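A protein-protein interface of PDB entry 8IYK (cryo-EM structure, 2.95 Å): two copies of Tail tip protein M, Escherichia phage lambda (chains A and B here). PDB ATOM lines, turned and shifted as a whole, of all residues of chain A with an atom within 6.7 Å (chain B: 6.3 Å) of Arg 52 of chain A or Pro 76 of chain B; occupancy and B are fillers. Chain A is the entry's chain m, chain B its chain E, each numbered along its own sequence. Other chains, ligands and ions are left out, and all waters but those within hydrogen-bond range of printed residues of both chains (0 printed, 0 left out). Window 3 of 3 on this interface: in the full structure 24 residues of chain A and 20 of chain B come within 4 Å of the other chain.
The backbone NH of Val 93 of chain A is in hydrogen-bond range of the backbone carbonyl oxygen of Met 12 of chain B, 3.3 Å away.
O of Ser 94 of chain A lies within hydrogen-bond range of NH1 of Arg 52 of chain A, 3.2 Å away.
O of Pro 76 of chain B touches NH2 of Arg 52 of chain A (3.7 Å). Ala 55 of chain A touches Tyr 77 of chain B. Thr 56 of chain A touches Glu 78 of chain B. Val 93 of chain A touches Tyr 77 of chain B.
Of the printed residues of chain B, Ala 55 of chain A touches Tyr 77 (3.7 Å). Printed residues of chain B within 4 Å of Thr 56 of chain A: Glu 78 (3.5 Å). Of the printed residues of chain B, Val 93 of chain A touches Met 12 and Tyr 77. Printed residues of chain A within 4 Å of Met 12 of chain B: Val 93. Pro 76 of chain B touches just one residue of chain A: Arg 52. The nearest residue of chain B that does not touch Arg 52 of chain A is Trp 79 of chain B (4.05 Å). The nearest printed residue of chain A that does not touch Met 12 of chain B is Ser 94 of chain A (5.7 Å).
Of the 9 printed residues of chain B, 4 touch a printed residue of chain A. Hydrophobic or aromatic side chains of chain B within 4 Å of the printed part of chain A: Tyr 77. Of the 14 printed residues of chain A, 4 touch a printed residue of chain B. Hydrophobic or aromatic side chains of chain A within 4 Å of the printed part of chain B: Ala 55 and Val 93. Along chain A the printed residues that touch a printed residue of chain B span positions 52 to 93.
No position is printed for both chains. Of the 5 pairs that touch across the chains among the printed residues, none has its exchanged pair printed and touching as well.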
ATOM      1  N   VAL A  50     -19.341 -10.659 -23.697  1.00  0.00           N
ATOM      2  CA  VAL A  50     -19.568 -11.941 -23.030  1.00  0.00           C
ATOM      3  C   VAL A  50     -18.345 -12.822 -23.209  1.00  0.00           C
ATOM      4  O   VAL A  50     -17.633 -12.742 -24.219  1.00  0.00           O
ATOM      5  CB  VAL A  50     -20.824 -12.650 -23.595  1.00  0.00           C
ATOM      6  CG1 VAL A  50     -20.588 -13.159 -25.012  1.00  0.00           C
ATOM      7  CG2 VAL A  50     -21.323 -13.741 -22.674  1.00  0.00           C
ATOM      8  N   PRO A  51     -18.049 -13.656 -22.211  1.00  0.00           N
ATOM      9  CA  PRO A  51     -16.935 -14.602 -22.351  1.00  0.00           C
ATOM     10  C   PRO A  51     -17.096 -15.503 -23.567  1.00  0.00           C
ATOM     11  O   PRO A  51     -18.199 -15.735 -24.067  1.00  0.00           O
ATOM     12  CB  PRO A  51     -16.989 -15.407 -21.051  1.00  0.00           C
ATOM     13  CG  PRO A  51     -17.570 -14.466 -20.064  1.00  0.00           C
ATOM     14  CD  PRO A  51     -18.486 -13.531 -20.809  1.00  0.00           C
ATOM     15  N   ARG A  52     -15.956 -16.014 -24.047  1.00  0.00           N
ATOM     16  CA  ARG A  52     -15.941 -16.790 -25.285  1.00  0.00           C
ATOM     17  C   ARG A  52     -16.817 -18.033 -25.198  1.00  0.00           C
ATOM     18  O   ARG A  52     -17.307 -18.517 -26.224  1.00  0.00           O
ATOM     19  CB  ARG A  52     -14.509 -17.192 -25.641  1.00  0.00           C
ATOM     20  CG  ARG A  52     -13.544 -16.032 -25.772  1.00  0.00           C
ATOM     21  CD  ARG A  52     -13.332 -15.656 -27.225  1.00  0.00           C
ATOM     22  NE  ARG A  52     -12.741 -16.734 -28.008  1.00  0.00           N
ATOM     23  CZ  ARG A  52     -11.450 -17.032 -28.023  1.00  0.00           C
ATOM     24  NH1 ARG A  52     -10.575 -16.347 -27.307  1.00  0.00           N
ATOM     25  NH2 ARG A  52     -11.024 -18.039 -28.780  1.00  0.00           N
ATOM     26  N   GLU A  53     -17.020 -18.567 -23.993  1.00  0.00           N
ATOM     27  CA  GLU A  53     -17.794 -19.793 -23.848  1.00  0.00           C
ATOM     28  C   GLU A  53     -19.285 -19.561 -24.050  1.00  0.00           C
ATOM     29  O   GLU A  53     -19.973 -20.431 -24.596  1.00  0.00           O
ATOM     30  CB  GLU A  53     -17.549 -20.434 -22.476  1.00  0.00           C
ATOM     31  CG  GLU A  53     -16.089 -20.751 -22.109  1.00  0.00           C
ATOM     32  CD  GLU A  53     -15.184 -19.533 -22.039  1.00  0.00           C
ATOM     33  OE1 GLU A  53     -14.072 -19.587 -22.604  1.00  0.00           O
ATOM     34  OE2 GLU A  53     -15.586 -18.524 -21.421  1.00  0.00           O
ATOM     35  N   GLU A  54     -19.804 -18.411 -23.623  1.00  0.00           N
ATOM     36  CA  GLU A  54     -21.221 -18.101 -23.753  1.00  0.00           C
ATOM     37  C   GLU A  54     -21.573 -17.473 -25.094  1.00  0.00           C
ATOM     38  O   GLU A  54     -22.758 -17.239 -25.364  1.00  0.00           O
ATOM     39  CB  GLU A  54     -21.662 -17.167 -22.625  1.00  0.00           C
ATOM     40  CG  GLU A  54     -20.794 -17.241 -21.382  1.00  0.00           C
ATOM     41  CD  GLU A  54     -21.507 -16.731 -20.146  1.00  0.00           C
ATOM     42  OE1 GLU A  54     -22.481 -15.964 -20.297  1.00  0.00           O
ATOM     43  OE2 GLU A  54     -21.097 -17.097 -19.025  1.00  0.00           O
ATOM     44  N   ALA A  55     -20.576 -17.185 -25.933  1.00  0.00           N
ATOM     45  CA  ALA A  55     -20.860 -16.664 -27.265  1.00  0.00           C
ATOM     46  C   ALA A  55     -21.654 -17.671 -28.082  1.00  0.00           C
ATOM     47  O   ALA A  55     -22.552 -17.295 -28.844  1.00  0.00           O
ATOM     48  CB  ALA A  55     -19.559 -16.304 -27.977  1.00  0.00           C
ATOM     49  N   THR A  56     -21.335 -18.958 -27.934  1.00  0.00           N
ATOM     50  CA  THR A  56     -22.079 -19.990 -28.645  1.00  0.00           C
ATOM     51  C   THR A  56     -23.542 -19.997 -28.225  1.00  0.00           C
ATOM     52  O   THR A  56     -24.434 -20.112 -29.070  1.00  0.00           O
ATOM     53  CB  THR A  56     -21.448 -21.359 -28.402  1.00  0.00           C
ATOM     54  OG1 THR A  56     -21.949 -21.906 -27.177  1.00  0.00           O
ATOM     55  CG2 THR A  56     -19.934 -21.241 -28.320  1.00  0.00           C
ATOM     56  N   VAL A  57     -23.808 -19.862 -26.926  1.00  0.00           N
ATOM     57  CA  VAL A  57     -25.187 -19.847 -26.444  1.00  0.00           C
ATOM     58  C   VAL A  57     -25.924 -18.611 -26.949  1.00  0.00           C
ATOM     59  O   VAL A  57     -27.078 -18.697 -27.395  1.00  0.00           O
ATOM     60  CB  VAL A  57     -25.210 -19.932 -24.909  1.00  0.00           C
ATOM     61  CG1 VAL A  57     -26.623 -19.746 -24.387  1.00  0.00           C
ATOM     62  CG2 VAL A  57     -24.635 -21.258 -24.448  1.00  0.00           C
ATOM     63  N   VAL A  93     -14.604 -11.446 -31.957  1.00  0.00           N
ATOM     64  CA  VAL A  93     -14.130 -12.459 -31.020  1.00  0.00           C
ATOM     65  C   VAL A  93     -12.702 -12.169 -30.578  1.00  0.00           C
ATOM     66  O   VAL A  93     -11.745 -12.635 -31.203  1.00  0.00           O
ATOM     67  CB  VAL A  93     -14.226 -13.856 -31.657  1.00  0.00           C
ATOM     68  CG1 VAL A  93     -13.903 -14.935 -30.645  1.00  0.00           C
ATOM     69  CG2 VAL A  93     -15.603 -14.069 -32.251  1.00  0.00           C
ATOM     70  N   SER A  94     -12.543 -11.449 -29.470  1.00  0.00           N
ATOM     71  CA  SER A  94     -11.219 -11.065 -28.992  1.00  0.00           C
ATOM     72  C   SER A  94     -10.539 -12.259 -28.325  1.00  0.00           C
ATOM     73  O   SER A  94     -11.020 -13.394 -28.381  1.00  0.00           O
ATOM     74  CB  SER A  94     -11.323  -9.870 -28.049  1.00  0.00           C
ATOM     75  OG  SER A  94     -11.856 -10.259 -26.796  1.00  0.00           O
ATOM     76  N   MET A  95      -9.394 -12.011 -27.683  1.00  0.00           N
ATOM     77  CA  MET A  95      -8.609 -13.098 -27.105  1.00  0.00           C
ATOM     78  C   MET A  95      -9.357 -13.799 -25.979  1.00  0.00           C
ATOM     79  O   MET A  95      -9.307 -15.029 -25.867  1.00  0.00           O
ATOM     80  CB  MET A  95      -7.268 -12.568 -26.601  1.00  0.00           C
ATOM     81  CG  MET A  95      -6.115 -12.759 -27.570  1.00  0.00           C
ATOM     82  SD  MET A  95      -6.303 -14.225 -28.598  1.00  0.00           S
ATOM     83  CE  MET A  95      -5.352 -15.417 -27.661  1.00  0.00           C
ATOM     84  N   LEU A  96     -10.055 -13.040 -25.132  1.00  0.00           N
ATOM     85  CA  LEU A  96     -10.747 -13.610 -23.986  1.00  0.00           C
ATOM     86  C   LEU A  96     -12.241 -13.330 -23.950  1.00  0.00           C
ATOM     87  O   LEU A  96     -12.964 -14.052 -23.256  1.00  0.00           O
ATOM     88  CB  LEU A  96     -10.124 -13.103 -22.675  1.00  0.00           C
ATOM     89  CG  LEU A  96      -8.889 -13.855 -22.182  1.00  0.00           C
ATOM     90  CD1 LEU A  96      -8.087 -12.989 -21.230  1.00  0.00           C
ATOM     91  CD2 LEU A  96      -9.285 -15.160 -21.520  1.00  0.00           C
ATOM     92  N   ARG A  97     -12.722 -12.316 -24.662  1.00  0.00           N
ATOM     93  CA  ARG A  97     -14.132 -11.961 -24.672  1.00  0.00           C
ATOM     94  C   ARG A  97     -14.588 -11.748 -26.107  1.00  0.00           C
ATOM     95  O   ARG A  97     -13.779 -11.586 -27.022  1.00  0.00           O
ATOM     96  CB  ARG A  97     -14.398 -10.700 -23.842  1.00  0.00           C
ATOM     97  CG  ARG A  97     -14.314 -10.915 -22.346  1.00  0.00           C
ATOM     98  CD  ARG A  97     -14.602  -9.627 -21.602  1.00  0.00           C
ATOM     99  NE  ARG A  97     -15.998  -9.527 -21.191  1.00  0.00           N
ATOM    100  CZ  ARG A  97     -16.554 -10.251 -20.231  1.00  0.00           C
ATOM    101  NH1 ARG A  97     -15.858 -11.144 -19.545  1.00  0.00           N
ATOM    102  NH2 ARG A  97     -17.839 -10.071 -19.944  1.00  0.00           N
ATOM    103  N   VAL A  98     -15.903 -11.754 -26.300  1.00  0.00           N
ATOM    104  CA  VAL A  98     -16.509 -11.489 -27.595  1.00  0.00           C
ATOM    105  C   VAL A  98     -17.580 -10.425 -27.411  1.00  0.00           C
ATOM    106  O   VAL A  98     -18.340 -10.451 -26.436  1.00  0.00           O
ATOM    107  CB  VAL A  98     -17.090 -12.774 -28.231  1.00  0.00           C
ATOM    108  CG1 VAL A  98     -16.953 -13.943 -27.281  1.00  0.00           C
ATOM    109  CG2 VAL A  98     -18.536 -12.582 -28.656  1.00  0.00           C
ATOM    110  N   VAL B   8      -5.845 -17.276 -36.925  1.00  0.00           N
ATOM    111  CA  VAL B   8      -6.296 -15.889 -37.014  1.00  0.00           C
ATOM    112  C   VAL B   8      -6.088 -15.215 -35.660  1.00  0.00           C
ATOM    113  O   VAL B   8      -6.559 -15.708 -34.627  1.00  0.00           O
ATOM    114  CB  VAL B   8      -7.755 -15.806 -37.486  1.00  0.00           C
ATOM    115  CG1 VAL B   8      -7.874 -16.436 -38.851  1.00  0.00           C
ATOM    116  CG2 VAL B   8      -8.688 -16.527 -36.532  1.00  0.00           C
ATOM    117  N   MET B  12     -11.854 -11.583 -35.140  1.00  0.00           N
ATOM    118  CA  MET B  12     -12.512 -11.435 -36.424  1.00  0.00           C
ATOM    119  C   MET B  12     -13.926 -10.889 -36.250  1.00  0.00           C
ATOM    120  O   MET B  12     -14.448 -10.774 -35.141  1.00  0.00           O
ATOM    121  CB  MET B  12     -12.538 -12.778 -37.147  1.00  0.00           C
ATOM    122  CG  MET B  12     -12.634 -13.963 -36.207  1.00  0.00           C
ATOM    123  SD  MET B  12     -12.818 -15.529 -37.071  1.00  0.00           S
ATOM    124  CE  MET B  12     -13.599 -16.517 -35.802  1.00  0.00           C
ATOM    125  N   TRP B  73     -12.473 -25.587 -42.679  1.00  0.00           N
ATOM    126  CA  TRP B  73     -11.877 -24.693 -41.699  1.00  0.00           C
ATOM    127  C   TRP B  73     -12.670 -24.791 -40.408  1.00  0.00           C
ATOM    128  O   TRP B  73     -13.900 -24.833 -40.434  1.00  0.00           O
ATOM    129  CB  TRP B  73     -11.856 -23.246 -42.201  1.00  0.00           C
ATOM    130  CG  TRP B  73     -11.325 -22.266 -41.199  1.00  0.00           C
ATOM    131  CD1 TRP B  73     -10.182 -22.381 -40.466  1.00  0.00           C
ATOM    132  CD2 TRP B  73     -11.918 -21.018 -40.822  1.00  0.00           C
ATOM    133  NE1 TRP B  73     -10.025 -21.284 -39.657  1.00  0.00           N
ATOM    134  CE2 TRP B  73     -11.079 -20.432 -39.856  1.00  0.00           C
ATOM    135  CE3 TRP B  73     -13.078 -20.340 -41.206  1.00  0.00           C
ATOM    136  CZ2 TRP B  73     -11.361 -19.203 -39.270  1.00  0.00           C
ATOM    137  CZ3 TRP B  73     -13.355 -19.119 -40.622  1.00  0.00           C
ATOM    138  CH2 TRP B  73     -12.501 -18.564 -39.665  1.00  0.00           C
ATOM    139  N   THR B  74     -11.960 -24.831 -39.284  1.00  0.00           N
ATOM    140  CA  THR B  74     -12.605 -24.829 -37.976  1.00  0.00           C
ATOM    141  C   THR B  74     -12.433 -23.450 -37.361  1.00  0.00           C
ATOM    142  O   THR B  74     -11.348 -23.128 -36.853  1.00  0.00           O
ATOM    143  CB  THR B  74     -12.008 -25.904 -37.064  1.00  0.00           C
ATOM    144  OG1 THR B  74     -12.091 -27.180 -37.710  1.00  0.00           O
ATOM    145  CG2 THR B  74     -12.759 -25.961 -35.749  1.00  0.00           C
ATOM    146  N   PRO B  75     -13.459 -22.598 -37.386  1.00  0.00           N
ATOM    147  CA  PRO B  75     -13.284 -21.238 -36.885  1.00  0.00           C
ATOM    148  C   PRO B  75     -13.061 -21.244 -35.385  1.00  0.00           C
ATOM    149  O   PRO B  75     -13.633 -22.079 -34.662  1.00  0.00           O
ATOM    150  CB  PRO B  75     -14.610 -20.547 -37.254  1.00  0.00           C
ATOM    151  CG  PRO B  75     -15.469 -21.576 -37.910  1.00  0.00           C
ATOM    152  CD  PRO B  75     -14.856 -22.910 -37.717  1.00  0.00           C
ATOM    153  N   PRO B  76     -12.241 -20.332 -34.868  1.00  0.00           N
ATOM    154  CA  PRO B  76     -12.067 -20.251 -33.414  1.00  0.00           C
ATOM    155  C   PRO B  76     -13.218 -19.515 -32.753  1.00  0.00           C
ATOM    156  O   PRO B  76     -13.013 -18.703 -31.847  1.00  0.00           O
ATOM    157  CB  PRO B  76     -10.747 -19.480 -33.257  1.00  0.00           C
ATOM    158  CG  PRO B  76     -10.176 -19.349 -34.648  1.00  0.00           C
ATOM    159  CD  PRO B  76     -11.332 -19.426 -35.579  1.00  0.00           C
ATOM    160  N   TYR B  77     -14.435 -19.795 -33.207  1.00  0.00           N
ATOM    161  CA  TYR B  77     -15.637 -19.172 -32.672  1.00  0.00           C
ATOM    162  C   TYR B  77     -16.601 -20.189 -32.087  1.00  0.00           C
ATOM    163  O   TYR B  77     -17.025 -20.046 -30.934  1.00  0.00           O
ATOM    164  CB  TYR B  77     -16.319 -18.359 -33.780  1.00  0.00           C
ATOM    165  CG  TYR B  77     -17.373 -17.400 -33.294  1.00  0.00           C
ATOM    166  CD1 TYR B  77     -17.475 -17.060 -31.952  1.00  0.00           C
ATOM    167  CD2 TYR B  77     -18.256 -16.818 -34.184  1.00  0.00           C
ATOM    168  CE1 TYR B  77     -18.435 -16.177 -31.514  1.00  0.00           C
ATOM    169  CE2 TYR B  77     -19.209 -15.932 -33.759  1.00  0.00           C
ATOM    170  CZ  TYR B  77     -19.299 -15.614 -32.423  1.00  0.00           C
ATOM    171  OH  TYR B  77     -20.264 -14.731 -32.000  1.00  0.00           O
ATOM    172  N   GLU B  78     -16.961 -21.216 -32.855  1.00  0.00           N
ATOM    173  CA  GLU B  78     -17.813 -22.295 -32.379  1.00  0.00           C
ATOM    174  C   GLU B  78     -17.119 -23.646 -32.389  1.00  0.00           C
ATOM    175  O   GLU B  78     -17.675 -24.611 -31.852  1.00  0.00           O
ATOM    176  CB  GLU B  78     -19.090 -22.380 -33.225  1.00  0.00           C
ATOM    177  CG  GLU B  78     -19.683 -21.033 -33.597  1.00  0.00           C
ATOM    178  CD  GLU B  78     -20.610 -20.491 -32.529  1.00  0.00           C
ATOM    179  OE1 GLU B  78     -20.112 -19.866 -31.570  1.00  0.00           O
ATOM    180  OE2 GLU B  78     -21.836 -20.694 -32.647  1.00  0.00           O
ATOM    181  N   TRP B  79     -15.931 -23.740 -32.989  1.00  0.00           N
ATOM    182  CA  TRP B  79     -15.143 -24.971 -33.034  1.00  0.00           C
ATOM    183  C   TRP B  79     -15.892 -26.103 -33.731  1.00  0.00           C
ATOM    184  O   TRP B  79     -15.763 -27.271 -33.359  1.00  0.00           O
ATOM    185  CB  TRP B  79     -14.700 -25.392 -31.632  1.00  0.00           C
ATOM    186  CG  TRP B  79     -14.110 -24.259 -30.858  1.00  0.00           C
ATOM    187  CD1 TRP B  79     -14.703 -23.556 -29.852  1.00  0.00           C
ATOM    188  CD2 TRP B  79     -12.814 -23.680 -31.043  1.00  0.00           C
ATOM    189  NE1 TRP B  79     -13.852 -22.582 -29.390  1.00  0.00           N
ATOM    190  CE2 TRP B  79     -12.685 -22.637 -30.107  1.00  0.00           C
ATOM    191  CE3 TRP B  79     -11.748 -23.946 -31.907  1.00  0.00           C
ATOM    192  CZ2 TRP B  79     -11.536 -21.861 -30.009  1.00  0.00           C
ATOM    193  CZ3 TRP B  79     -10.608 -23.174 -31.808  1.00  0.00           C
ATOM    194  CH2 TRP B  79     -10.509 -22.146 -30.865  1.00  0.00           C
